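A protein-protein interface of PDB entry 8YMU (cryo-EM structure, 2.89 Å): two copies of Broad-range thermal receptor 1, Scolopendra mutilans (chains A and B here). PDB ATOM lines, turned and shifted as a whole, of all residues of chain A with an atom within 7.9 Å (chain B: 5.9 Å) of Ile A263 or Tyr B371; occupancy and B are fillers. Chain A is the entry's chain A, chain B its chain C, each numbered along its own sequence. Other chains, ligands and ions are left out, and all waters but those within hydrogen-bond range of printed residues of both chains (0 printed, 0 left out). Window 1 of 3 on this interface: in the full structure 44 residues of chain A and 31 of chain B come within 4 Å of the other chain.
OH of Tyr A265 is in hydrogen-bond range of OH of Tyr B371 (3.1 Å).
The backbone carbonyl oxygen (O) of Cys A341 sits close to the backbone carbonyl oxygen (O) of Ile A263, at 2.5 Å. The side-chain sulfur (SG) of Cys A273 is disulfide-bonded to the side-chain sulfur (SG) of Cys A341, 2.0 Å away. The backbone carbonyl oxygen of Cys A341 sits at hydrogen-bond distance from the backbone NH of Tyr A265 (3.1 Å). The side-chain amino group (NZ) of Lys A340 lies within salt-bridge range of the side-chain carboxylate (OE2) of Glu A343, 3.7 Å away. O of Ile A263 lies within hydrogen-bond range of N of Glu A343 (2.9 Å). N of Leu A345 is in hydrogen-bond range of O of Thr A261 (2.9 Å).
CD1 of Ile A263 touches CB of Phe B92 (3.6 Å). Ile A263 touches Tyr B371. OH of Tyr B371 touches CG of Glu A343, at 3.4 Å. Leu A345 touches Tyr B371. Phe B92 touches Gln A373. Gln A373 touches Gln B373 (NE2 to NE2, 3.6 Å).
Ile A263 touches two residues of chain B. Tyr B371 touches four residues of chain A. Printed residues of chain B within 4 Å of Gln A373: Phe B92 and Gln B373. Printed residues of chain A within 4 Å of Phe B92: Ile A263 (3.6 Å) and Gln A373 (3.8 Å). Of the printed residues of chain B, Tyr A265 touches Tyr B371 (3.1 Å). Printed residues of chain A within 4 Å of Gln B373: Gln A373 (3.6 Å). The nearest residue of chain A that does not touch Tyr B371 is Arg A339 (5.2 Å). The nearest printed residue of chain A that does not touch Gln B373 is Thr A261 (7.6 Å).
Of the 11 printed residues of chain B, 3 touch a printed residue of chain A. Hydrophobic or aromatic side chains of chain B that line the printed part of chain A: Phe B92 and Tyr B371. Hydrophobic or aromatic side chains of chain A that line the printed part of chain B: Ile A263, Tyr A265 and Leu A345. Along chain A the printed residues that touch a printed residue of chain B span positions 263 to 373. Among the printed residues, 7 pairs touch across the chains. Among the printed residues, no Asp or Glu carboxylate lies within 4 Å of a Lys or Arg side-chain nitrogen of the other chain.
Gln B373 touches its own counterpart, Gln A373. Positions printed for both chains: 260, 372 and 373. Of the 7 pairs that touch across the chains among the printed residues, 1 has its exchanged pair printed and touching as well.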
ATOM      1  N   VAL A  88      35.278   0.186  25.130  1.00  0.00           N
ATOM      2  CA  VAL A  88      34.770  -0.560  26.276  1.00  0.00           C
ATOM      3  C   VAL A  88      35.929  -0.884  27.205  1.00  0.00           C
ATOM      4  O   VAL A  88      36.893  -1.544  26.802  1.00  0.00           O
ATOM      5  CB  VAL A  88      34.047  -1.843  25.833  1.00  0.00           C
ATOM      6  CG1 VAL A  88      33.742  -2.726  27.030  1.00  0.00           C
ATOM      7  CG2 VAL A  88      32.776  -1.497  25.087  1.00  0.00           C
ATOM      8  N   PHE A 260      26.826 -11.933  38.142  1.00  0.00           N
ATOM      9  CA  PHE A 260      26.343 -10.669  37.615  1.00  0.00           C
ATOM     10  C   PHE A 260      27.326 -10.102  36.602  1.00  0.00           C
ATOM     11  O   PHE A 260      28.539 -10.078  36.827  1.00  0.00           O
ATOM     12  CB  PHE A 260      26.129  -9.654  38.737  1.00  0.00           C
ATOM     13  CG  PHE A 260      25.242 -10.147  39.835  1.00  0.00           C
ATOM     14  CD1 PHE A 260      23.892 -10.328  39.619  1.00  0.00           C
ATOM     15  CD2 PHE A 260      25.760 -10.437  41.084  1.00  0.00           C
ATOM     16  CE1 PHE A 260      23.073 -10.782  40.624  1.00  0.00           C
ATOM     17  CE2 PHE A 260      24.944 -10.892  42.094  1.00  0.00           C
ATOM     18  CZ  PHE A 260      23.599 -11.066  41.864  1.00  0.00           C
ATOM     19  N   THR A 261      26.783  -9.661  35.474  1.00  0.00           N
ATOM     20  CA  THR A 261      27.504  -8.824  34.530  1.00  0.00           C
ATOM     21  C   THR A 261      26.730  -7.526  34.376  1.00  0.00           C
ATOM     22  O   THR A 261      25.502  -7.508  34.462  1.00  0.00           O
ATOM     23  CB  THR A 261      27.680  -9.508  33.166  1.00  0.00           C
ATOM     24  OG1 THR A 261      28.245 -10.812  33.348  1.00  0.00           O
ATOM     25  CG2 THR A 261      28.586  -8.685  32.261  1.00  0.00           C
ATOM     26  N   GLN A 262      27.454  -6.434  34.177  1.00  0.00           N
ATOM     27  CA  GLN A 262      26.845  -5.118  34.072  1.00  0.00           C
ATOM     28  C   GLN A 262      27.418  -4.407  32.860  1.00  0.00           C
ATOM     29  O   GLN A 262      28.601  -4.061  32.842  1.00  0.00           O
ATOM     30  CB  GLN A 262      27.090  -4.300  35.341  1.00  0.00           C
ATOM     31  CG  GLN A 262      26.204  -3.082  35.474  1.00  0.00           C
ATOM     32  CD  GLN A 262      26.421  -2.355  36.782  1.00  0.00           C
ATOM     33  OE1 GLN A 262      26.676  -1.152  36.801  1.00  0.00           O
ATOM     34  NE2 GLN A 262      26.322  -3.084  37.886  1.00  0.00           N
ATOM     35  N   ILE A 263      26.576  -4.184  31.857  1.00  0.00           N
ATOM     36  CA  ILE A 263      26.976  -3.511  30.629  1.00  0.00           C
ATOM     37  C   ILE A 263      26.473  -2.079  30.709  1.00  0.00           C
ATOM     38  O   ILE A 263      25.262  -1.842  30.786  1.00  0.00           O
ATOM     39  CB  ILE A 263      26.430  -4.229  29.387  1.00  0.00           C
ATOM     40  CG1 ILE A 263      26.982  -5.655  29.331  1.00  0.00           C
ATOM     41  CG2 ILE A 263      26.802  -3.468  28.126  1.00  0.00           C
ATOM     42  CD1 ILE A 263      26.321  -6.526  28.307  1.00  0.00           C
ATOM     43  N   ASN A 264      27.399  -1.128  30.709  1.00  0.00           N
ATOM     44  CA  ASN A 264      27.086   0.291  30.800  1.00  0.00           C
ATOM     45  C   ASN A 264      27.321   0.912  29.430  1.00  0.00           C
ATOM     46  O   ASN A 264      28.416   0.800  28.870  1.00  0.00           O
ATOM     47  CB  ASN A 264      27.935   0.970  31.871  1.00  0.00           C
ATOM     48  CG  ASN A 264      27.596   0.496  33.267  1.00  0.00           C
ATOM     49  OD1 ASN A 264      26.625   0.952  33.870  1.00  0.00           O
ATOM     50  ND2 ASN A 264      28.394  -0.426  33.790  1.00  0.00           N
ATOM     51  N   TYR A 265      26.290   1.553  28.891  1.00  0.00           N
ATOM     52  CA  TYR A 265      26.369   2.188  27.587  1.00  0.00           C
ATOM     53  C   TYR A 265      26.523   3.693  27.748  1.00  0.00           C
ATOM     54  O   TYR A 265      26.003   4.284  28.698  1.00  0.00           O
ATOM     55  CB  TYR A 265      25.124   1.875  26.759  1.00  0.00           C
ATOM     56  CG  TYR A 265      24.931   0.403  26.481  1.00  0.00           C
ATOM     57  CD1 TYR A 265      25.641  -0.231  25.473  1.00  0.00           C
ATOM     58  CD2 TYR A 265      24.037  -0.352  27.226  1.00  0.00           C
ATOM     59  CE1 TYR A 265      25.466  -1.574  25.215  1.00  0.00           C
ATOM     60  CE2 TYR A 265      23.856  -1.695  26.975  1.00  0.00           C
ATOM     61  CZ  TYR A 265      24.573  -2.301  25.967  1.00  0.00           C
ATOM     62  OH  TYR A 265      24.399  -3.640  25.709  1.00  0.00           O
ATOM     63  N   ALA A 266      27.246   4.306  26.817  1.00  0.00           N
ATOM     64  CA  ALA A 266      27.467   5.743  26.855  1.00  0.00           C
ATOM     65  C   ALA A 266      26.272   6.480  26.268  1.00  0.00           C
ATOM     66  O   ALA A 266      25.722   6.083  25.237  1.00  0.00           O
ATOM     67  CB  ALA A 266      28.737   6.108  26.088  1.00  0.00           C
ATOM     68  N   CYS A 273      20.819   6.841  26.168  1.00  0.00           N
ATOM     69  CA  CYS A 273      20.209   6.035  27.216  1.00  0.00           C
ATOM     70  C   CYS A 273      18.901   6.653  27.682  1.00  0.00           C
ATOM     71  O   CYS A 273      18.530   7.756  27.274  1.00  0.00           O
ATOM     72  CB  CYS A 273      21.140   5.912  28.418  1.00  0.00           C
ATOM     73  SG  CYS A 273      22.543   4.828  28.266  1.00  0.00           S
ATOM     74  N   ARG A 339      18.082   1.844  24.555  1.00  0.00           N
ATOM     75  CA  ARG A 339      18.839   1.000  25.470  1.00  0.00           C
ATOM     76  C   ARG A 339      19.129   1.689  26.796  1.00  0.00           C
ATOM     77  O   ARG A 339      19.575   2.839  26.826  1.00  0.00           O
ATOM     78  CB  ARG A 339      20.161   0.567  24.830  1.00  0.00           C
ATOM     79  CG  ARG A 339      21.081   1.721  24.458  1.00  0.00           C
ATOM     80  CD  ARG A 339      22.400   1.241  23.872  1.00  0.00           C
ATOM     81  NE  ARG A 339      22.230   0.556  22.595  1.00  0.00           N
ATOM     82  CZ  ARG A 339      22.314  -0.756  22.419  1.00  0.00           C
ATOM     83  NH1 ARG A 339      22.555  -1.580  23.426  1.00  0.00           N
ATOM     84  NH2 ARG A 339      22.151  -1.257  21.198  1.00  0.00           N
ATOM     85  N   LYS A 340      18.862   0.992  27.893  1.00  0.00           N
ATOM     86  CA  LYS A 340      19.355   1.374  29.208  1.00  0.00           C
ATOM     87  C   LYS A 340      20.876   1.417  29.206  1.00  0.00           C
ATOM     88  O   LYS A 340      21.526   0.551  28.614  1.00  0.00           O
ATOM     89  CB  LYS A 340      18.865   0.355  30.238  1.00  0.00           C
ATOM     90  CG  LYS A 340      17.356   0.232  30.324  1.00  0.00           C
ATOM     91  CD  LYS A 340      16.922  -0.780  31.378  1.00  0.00           C
ATOM     92  CE  LYS A 340      17.271  -2.212  30.998  1.00  0.00           C
ATOM     93  NZ  LYS A 340      17.130  -3.128  32.163  1.00  0.00           N
ATOM     94  N   CYS A 341      21.458   2.420  29.865  1.00  0.00           N
ATOM     95  CA  CYS A 341      22.891   2.347  30.128  1.00  0.00           C
ATOM     96  C   CYS A 341      23.205   1.072  30.893  1.00  0.00           C
ATOM     97  O   CYS A 341      23.899   0.192  30.380  1.00  0.00           O
ATOM     98  CB  CYS A 341      23.404   3.553  30.918  1.00  0.00           C
ATOM     99  SG  CYS A 341      23.422   5.143  30.064  1.00  0.00           S
ATOM    100  N   GLU A 342      22.680   0.955  32.107  1.00  0.00           N
ATOM    101  CA  GLU A 342      22.953  -0.184  32.969  1.00  0.00           C
ATOM    102  C   GLU A 342      22.065  -1.352  32.566  1.00  0.00           C
ATOM    103  O   GLU A 342      20.860  -1.342  32.832  1.00  0.00           O
ATOM    104  CB  GLU A 342      22.717   0.178  34.437  1.00  0.00           C
ATOM    105  CG  GLU A 342      23.054  -0.932  35.418  1.00  0.00           C
ATOM    106  CD  GLU A 342      22.855  -0.513  36.860  1.00  0.00           C
ATOM    107  OE1 GLU A 342      22.432   0.638  37.093  1.00  0.00           O
ATOM    108  OE2 GLU A 342      23.114  -1.335  37.763  1.00  0.00           O
ATOM    109  N   GLU A 343      22.665  -2.349  31.921  1.00  0.00           N
ATOM    110  CA  GLU A 343      22.004  -3.606  31.590  1.00  0.00           C
ATOM    111  C   GLU A 343      22.600  -4.677  32.491  1.00  0.00           C
ATOM    112  O   GLU A 343      23.808  -4.939  32.436  1.00  0.00           O
ATOM    113  CB  GLU A 343      22.185  -3.954  30.114  1.00  0.00           C
ATOM    114  CG  GLU A 343      21.534  -5.263  29.696  1.00  0.00           C
ATOM    115  CD  GLU A 343      20.022  -5.173  29.630  1.00  0.00           C
ATOM    116  OE1 GLU A 343      19.499  -4.652  28.622  1.00  0.00           O
ATOM    117  OE2 GLU A 343      19.355  -5.630  30.583  1.00  0.00           O
ATOM    118  N   ASN A 344      21.759  -5.279  33.324  1.00  0.00           N
ATOM    119  CA  ASN A 344      22.195  -6.287  34.276  1.00  0.00           C
ATOM    120  C   ASN A 344      21.900  -7.680  33.738  1.00  0.00           C
ATOM    121  O   ASN A 344      20.757  -8.004  33.403  1.00  0.00           O
ATOM    122  CB  ASN A 344      21.502  -6.085  35.621  1.00  0.00           C
ATOM    123  CG  ASN A 344      22.154  -5.000  36.451  1.00  0.00           C
ATOM    124  OD1 ASN A 344      23.212  -5.210  37.044  1.00  0.00           O
ATOM    125  ND2 ASN A 344      21.530  -3.831  36.493  1.00  0.00           N
ATOM    126  N   LEU A 345      22.945  -8.496  33.654  1.00  0.00           N
ATOM    127  CA  LEU A 345      22.871  -9.845  33.121  1.00  0.00           C
ATOM    128  C   LEU A 345      23.097 -10.818  34.264  1.00  0.00           C
ATOM    129  O   LEU A 345      24.121 -10.744  34.950  1.00  0.00           O
ATOM    130  CB  LEU A 345      23.923 -10.064  32.033  1.00  0.00           C
ATOM    131  CG  LEU A 345      23.648  -9.502  30.641  1.00  0.00           C
ATOM    132  CD1 LEU A 345      23.628  -7.990  30.657  1.00  0.00           C
ATOM    133  CD2 LEU A 345      24.713 -10.006  29.691  1.00  0.00           C
ATOM    134  N   ILE A 372      32.068  -8.991  40.113  1.00  0.00           N
ATOM    135  CA  ILE A 372      31.112  -8.646  39.071  1.00  0.00           C
ATOM    136  C   ILE A 372      31.883  -8.097  37.884  1.00  0.00           C
ATOM    137  O   ILE A 372      32.697  -7.178  38.036  1.00  0.00           O
ATOM    138  CB  ILE A 372      30.077  -7.622  39.565  1.00  0.00           C
ATOM    139  CG1 ILE A 372      29.197  -8.238  40.650  1.00  0.00           C
ATOM    140  CG2 ILE A 372      29.226  -7.125  38.406  1.00  0.00           C
ATOM    141  CD1 ILE A 372      28.388  -7.229  41.416  1.00  0.00           C
ATOM    142  N   GLN A 373      31.647  -8.681  36.713  1.00  0.00           N
ATOM    143  CA  GLN A 373      32.137  -8.103  35.472  1.00  0.00           C
ATOM    144  C   GLN A 373      31.353  -6.839  35.156  1.00  0.00           C
ATOM    145  O   GLN A 373      30.120  -6.844  35.173  1.00  0.00           O
ATOM    146  CB  GLN A 373      31.992  -9.105  34.329  1.00  0.00           C
ATOM    147  CG  GLN A 373      32.934  -8.872  33.166  1.00  0.00           C
ATOM    148  CD  GLN A 373      33.164 -10.122  32.345  1.00  0.00           C
ATOM    149  OE1 GLN A 373      32.442 -11.109  32.482  1.00  0.00           O
ATOM    150  NE2 GLN A 373      34.163 -10.081  31.474  1.00  0.00           N
ATOM    151  N   VAL A 374      32.063  -5.753  34.878  1.00  0.00           N
ATOM    152  CA  VAL A 374      31.454  -4.484  34.504  1.00  0.00           C
ATOM    153  C   VAL A 374      32.144  -4.002  33.240  1.00  0.00           C
ATOM    154  O   VAL A 374      33.330  -3.655  33.270  1.00  0.00           O
ATOM    155  CB  VAL A 374      31.567  -3.437  35.624  1.00  0.00           C
ATOM    156  CG1 VAL A 374      30.759  -2.202  35.274  1.00  0.00           C
ATOM    157  CG2 VAL A 374      31.102  -4.016  36.949  1.00  0.00           C
ATOM    158  N   ALA A 375      31.408  -3.987  32.134  1.00  0.00           N
ATOM    159  CA  ALA A 375      31.909  -3.513  30.850  1.00  0.00           C
ATOM    160  C   ALA A 375      31.241  -2.180  30.553  1.00  0.00           C
ATOM    161  O   ALA A 375      30.048  -2.139  30.240  1.00  0.00           O
ATOM    162  CB  ALA A 375      31.624  -4.528  29.746  1.00  0.00           C
ATOM    163  N   THR A 376      32.000  -1.093  30.652  1.00  0.00           N
ATOM    164  CA  THR A 376      31.480   0.253  30.444  1.00  0.00           C
ATOM    165  C   THR A 376      32.077   0.819  29.166  1.00  0.00           C
ATOM    166  O   THR A 376      33.301   0.849  29.014  1.00  0.00           O
ATOM    167  CB  THR A 376      31.813   1.158  31.631  1.00  0.00           C
ATOM    168  OG1 THR A 376      31.282   0.591  32.834  1.00  0.00           O
ATOM    169  CG2 THR A 376      31.226   2.545  31.429  1.00  0.00           C
ATOM    170  N   GLU A 377      31.221   1.268  28.252  1.00  0.00           N
ATOM    171  CA  GLU A 377      31.688   1.918  27.037  1.00  0.00           C
ATOM    172  C   GLU A 377      31.697   3.423  27.263  1.00  0.00           C
ATOM    173  O   GLU A 377      30.701   3.997  27.718  1.00  0.00           O
ATOM    174  CB  GLU A 377      30.819   1.551  25.834  1.00  0.00           C
ATOM    175  CG  GLU A 377      29.583   2.398  25.644  1.00  0.00           C
ATOM    176  CD  GLU A 377      28.713   1.895  24.511  1.00  0.00           C
ATOM    177  OE1 GLU A 377      29.023   0.820  23.958  1.00  0.00           O
ATOM    178  OE2 GLU A 377      27.721   2.573  24.171  1.00  0.00           O
ATOM    179  N   PHE B  92      30.695  -6.830  24.573  1.00  0.00           N
ATOM    180  CA  PHE B  92      29.575  -7.733  24.818  1.00  0.00           C
ATOM    181  C   PHE B  92      28.478  -7.349  23.832  1.00  0.00           C
ATOM    182  O   PHE B  92      27.714  -6.411  24.076  1.00  0.00           O
ATOM    183  CB  PHE B  92      29.098  -7.644  26.263  1.00  0.00           C
ATOM    184  CG  PHE B  92      29.875  -8.514  27.209  1.00  0.00           C
ATOM    185  CD1 PHE B  92      31.048  -8.056  27.786  1.00  0.00           C
ATOM    186  CD2 PHE B  92      29.438  -9.790  27.516  1.00  0.00           C
ATOM    187  CE1 PHE B  92      31.767  -8.854  28.654  1.00  0.00           C
ATOM    188  CE2 PHE B  92      30.154 -10.590  28.383  1.00  0.00           C
ATOM    189  CZ  PHE B  92      31.319 -10.122  28.951  1.00  0.00           C
ATOM    190  N   VAL B  93      28.408  -8.071  22.719  1.00  0.00           N
ATOM    191  CA  VAL B  93      27.502  -7.747  21.623  1.00  0.00           C
ATOM    192  C   VAL B  93      26.186  -8.470  21.862  1.00  0.00           C
ATOM    193  O   VAL B  93      26.161  -9.695  22.009  1.00  0.00           O
ATOM    194  CB  VAL B  93      28.106  -8.137  20.265  1.00  0.00           C
ATOM    195  CG1 VAL B  93      27.247  -7.605  19.131  1.00  0.00           C
ATOM    196  CG2 VAL B  93      29.528  -7.619  20.147  1.00  0.00           C
ATOM    197  N   ALA B  94      25.091  -7.713  21.904  1.00  0.00           N
ATOM    198  CA  ALA B  94      23.769  -8.306  22.055  1.00  0.00           C
ATOM    199  C   ALA B  94      23.304  -8.863  20.716  1.00  0.00           C
ATOM    200  O   ALA B  94      23.236  -8.133  19.721  1.00  0.00           O
ATOM    201  CB  ALA B  94      22.779  -7.269  22.575  1.00  0.00           C
ATOM    202  N   GLN B  95      22.988 -10.153  20.690  1.00  0.00           N
ATOM    203  CA  GLN B  95      22.573 -10.822  19.466  1.00  0.00           C
ATOM    204  C   GLN B  95      21.054 -10.881  19.374  1.00  0.00           C
ATOM    205  O   GLN B  95      20.375 -11.281  20.321  1.00  0.00           O
ATOM    206  CB  GLN B  95      23.145 -12.238  19.414  1.00  0.00           C
ATOM    207  CG  GLN B  95      24.657 -12.301  19.323  1.00  0.00           C
ATOM    208  CD  GLN B  95      25.193 -11.667  18.058  1.00  0.00           C
ATOM    209  OE1 GLN B  95      25.808 -10.602  18.096  1.00  0.00           O
ATOM    210  NE2 GLN B  95      24.959 -12.319  16.925  1.00  0.00           N
ATOM    211  N   LEU B  98      21.048 -15.757  17.084  1.00  0.00           N
ATOM    212  CA  LEU B  98      22.265 -16.404  17.544  1.00  0.00           C
ATOM    213  C   LEU B  98      22.717 -17.474  16.554  1.00  0.00           C
ATOM    214  O   LEU B  98      21.909 -18.126  15.890  1.00  0.00           O
ATOM    215  CB  LEU B  98      22.050 -17.015  18.928  1.00  0.00           C
ATOM    216  CG  LEU B  98      22.079 -15.996  20.067  1.00  0.00           C
ATOM    217  CD1 LEU B  98      21.174 -16.433  21.205  1.00  0.00           C
ATOM    218  CD2 LEU B  98      23.496 -15.779  20.563  1.00  0.00           C
ATOM    219  N   PHE B 260      28.462 -17.990  24.190  1.00  0.00           N
ATOM    220  CA  PHE B 260      29.445 -17.857  23.130  1.00  0.00           C
ATOM    221  C   PHE B 260      30.497 -16.822  23.499  1.00  0.00           C
ATOM    222  O   PHE B 260      30.180 -15.702  23.908  1.00  0.00           O
ATOM    223  CB  PHE B 260      28.781 -17.460  21.812  1.00  0.00           C
ATOM    224  CG  PHE B 260      27.686 -18.386  21.384  1.00  0.00           C
ATOM    225  CD1 PHE B 260      27.974 -19.675  20.983  1.00  0.00           C
ATOM    226  CD2 PHE B 260      26.368 -17.971  21.389  1.00  0.00           C
ATOM    227  CE1 PHE B 260      26.972 -20.530  20.588  1.00  0.00           C
ATOM    228  CE2 PHE B 260      25.361 -18.823  20.996  1.00  0.00           C
ATOM    229  CZ  PHE B 260      25.663 -20.103  20.596  1.00  0.00           C
ATOM    230  N   TYR B 369      21.449 -16.652  26.582  1.00  0.00           N
ATOM    231  CA  TYR B 369      22.231 -15.433  26.701  1.00  0.00           C
ATOM    232  C   TYR B 369      22.611 -14.964  25.307  1.00  0.00           C
ATOM    233  O   TYR B 369      23.388 -15.630  24.615  1.00  0.00           O
ATOM    234  CB  TYR B 369      23.480 -15.667  27.550  1.00  0.00           C
ATOM    235  CG  TYR B 369      23.186 -16.365  28.857  1.00  0.00           C
ATOM    236  CD1 TYR B 369      22.838 -15.645  29.990  1.00  0.00           C
ATOM    237  CD2 TYR B 369      23.251 -17.747  28.955  1.00  0.00           C
ATOM    238  CE1 TYR B 369      22.564 -16.280  31.183  1.00  0.00           C
ATOM    239  CE2 TYR B 369      22.982 -18.390  30.144  1.00  0.00           C
ATOM    240  CZ  TYR B 369      22.639 -17.652  31.255  1.00  0.00           C
ATOM    241  OH  TYR B 369      22.368 -18.293  32.441  1.00  0.00           O
ATOM    242  N   ASN B 370      22.059 -13.825  24.898  1.00  0.00           N
ATOM    243  CA  ASN B 370      22.345 -13.274  23.583  1.00  0.00           C
ATOM    244  C   ASN B 370      23.592 -12.406  23.575  1.00  0.00           C
ATOM    245  O   ASN B 370      24.085 -12.054  22.497  1.00  0.00           O
ATOM    246  CB  ASN B 370      21.151 -12.456  23.087  1.00  0.00           C
ATOM    247  CG  ASN B 370      20.748 -11.365  24.054  1.00  0.00           C
ATOM    248  OD1 ASN B 370      20.891 -11.513  25.266  1.00  0.00           O
ATOM    249  ND2 ASN B 370      20.234 -10.265  23.524  1.00  0.00           N
ATOM    250  N   TYR B 371      24.114 -12.057  24.745  1.00  0.00           N
ATOM    251  CA  TYR B 371      25.320 -11.245  24.837  1.00  0.00           C
ATOM    252  C   TYR B 371      26.538 -12.127  24.605  1.00  0.00           C
ATOM    253  O   TYR B 371      26.907 -12.929  25.467  1.00  0.00           O
ATOM    254  CB  TYR B 371      25.385 -10.564  26.199  1.00  0.00           C
ATOM    255  CG  TYR B 371      24.573  -9.296  26.273  1.00  0.00           C
ATOM    256  CD1 TYR B 371      25.069  -8.102  25.775  1.00  0.00           C
ATOM    257  CD2 TYR B 371      23.301  -9.296  26.826  1.00  0.00           C
ATOM    258  CE1 TYR B 371      24.328  -6.941  25.838  1.00  0.00           C
ATOM    259  CE2 TYR B 371      22.553  -8.140  26.892  1.00  0.00           C
ATOM    260  CZ  TYR B 371      23.071  -6.966  26.396  1.00  0.00           C
ATOM    261  OH  TYR B 371      22.328  -5.810  26.457  1.00  0.00           O
ATOM    262  N   ILE B 372      27.160 -11.983  23.439  1.00  0.00           N
ATOM    263  CA  ILE B 372      28.364 -12.721  23.082  1.00  0.00           C
ATOM    264  C   ILE B 372      29.564 -11.876  23.475  1.00  0.00           C
ATOM    265  O   ILE B 372      29.632 -10.687  23.139  1.00  0.00           O
ATOM    266  CB  ILE B 372      28.396 -13.062  21.581  1.00  0.00           C
ATOM    267  CG1 ILE B 372      27.225 -13.987  21.237  1.00  0.00           C
ATOM    268  CG2 ILE B 372      29.728 -13.711  21.207  1.00  0.00           C
ATOM    269  CD1 ILE B 372      27.224 -14.492  19.809  1.00  0.00           C
ATOM    270  N   GLN B 373      30.500 -12.485  24.198  1.00  0.00           N
ATOM    271  CA  GLN B 373      31.721 -11.798  24.587  1.00  0.00           C
ATOM    272  C   GLN B 373      32.772 -11.959  23.498  1.00  0.00           C
ATOM    273  O   GLN B 373      33.270 -13.062  23.260  1.00  0.00           O
ATOM    274  CB  GLN B 373      32.235 -12.356  25.912  1.00  0.00           C
ATOM    275  CG  GLN B 373      33.448 -11.641  26.471  1.00  0.00           C
ATOM    276  CD  GLN B 373      33.916 -12.240  27.781  1.00  0.00           C
ATOM    277  OE1 GLN B 373      33.334 -13.202  28.279  1.00  0.00           O
ATOM    278  NE2 GLN B 373      34.972 -11.671  28.348  1.00  0.00           N
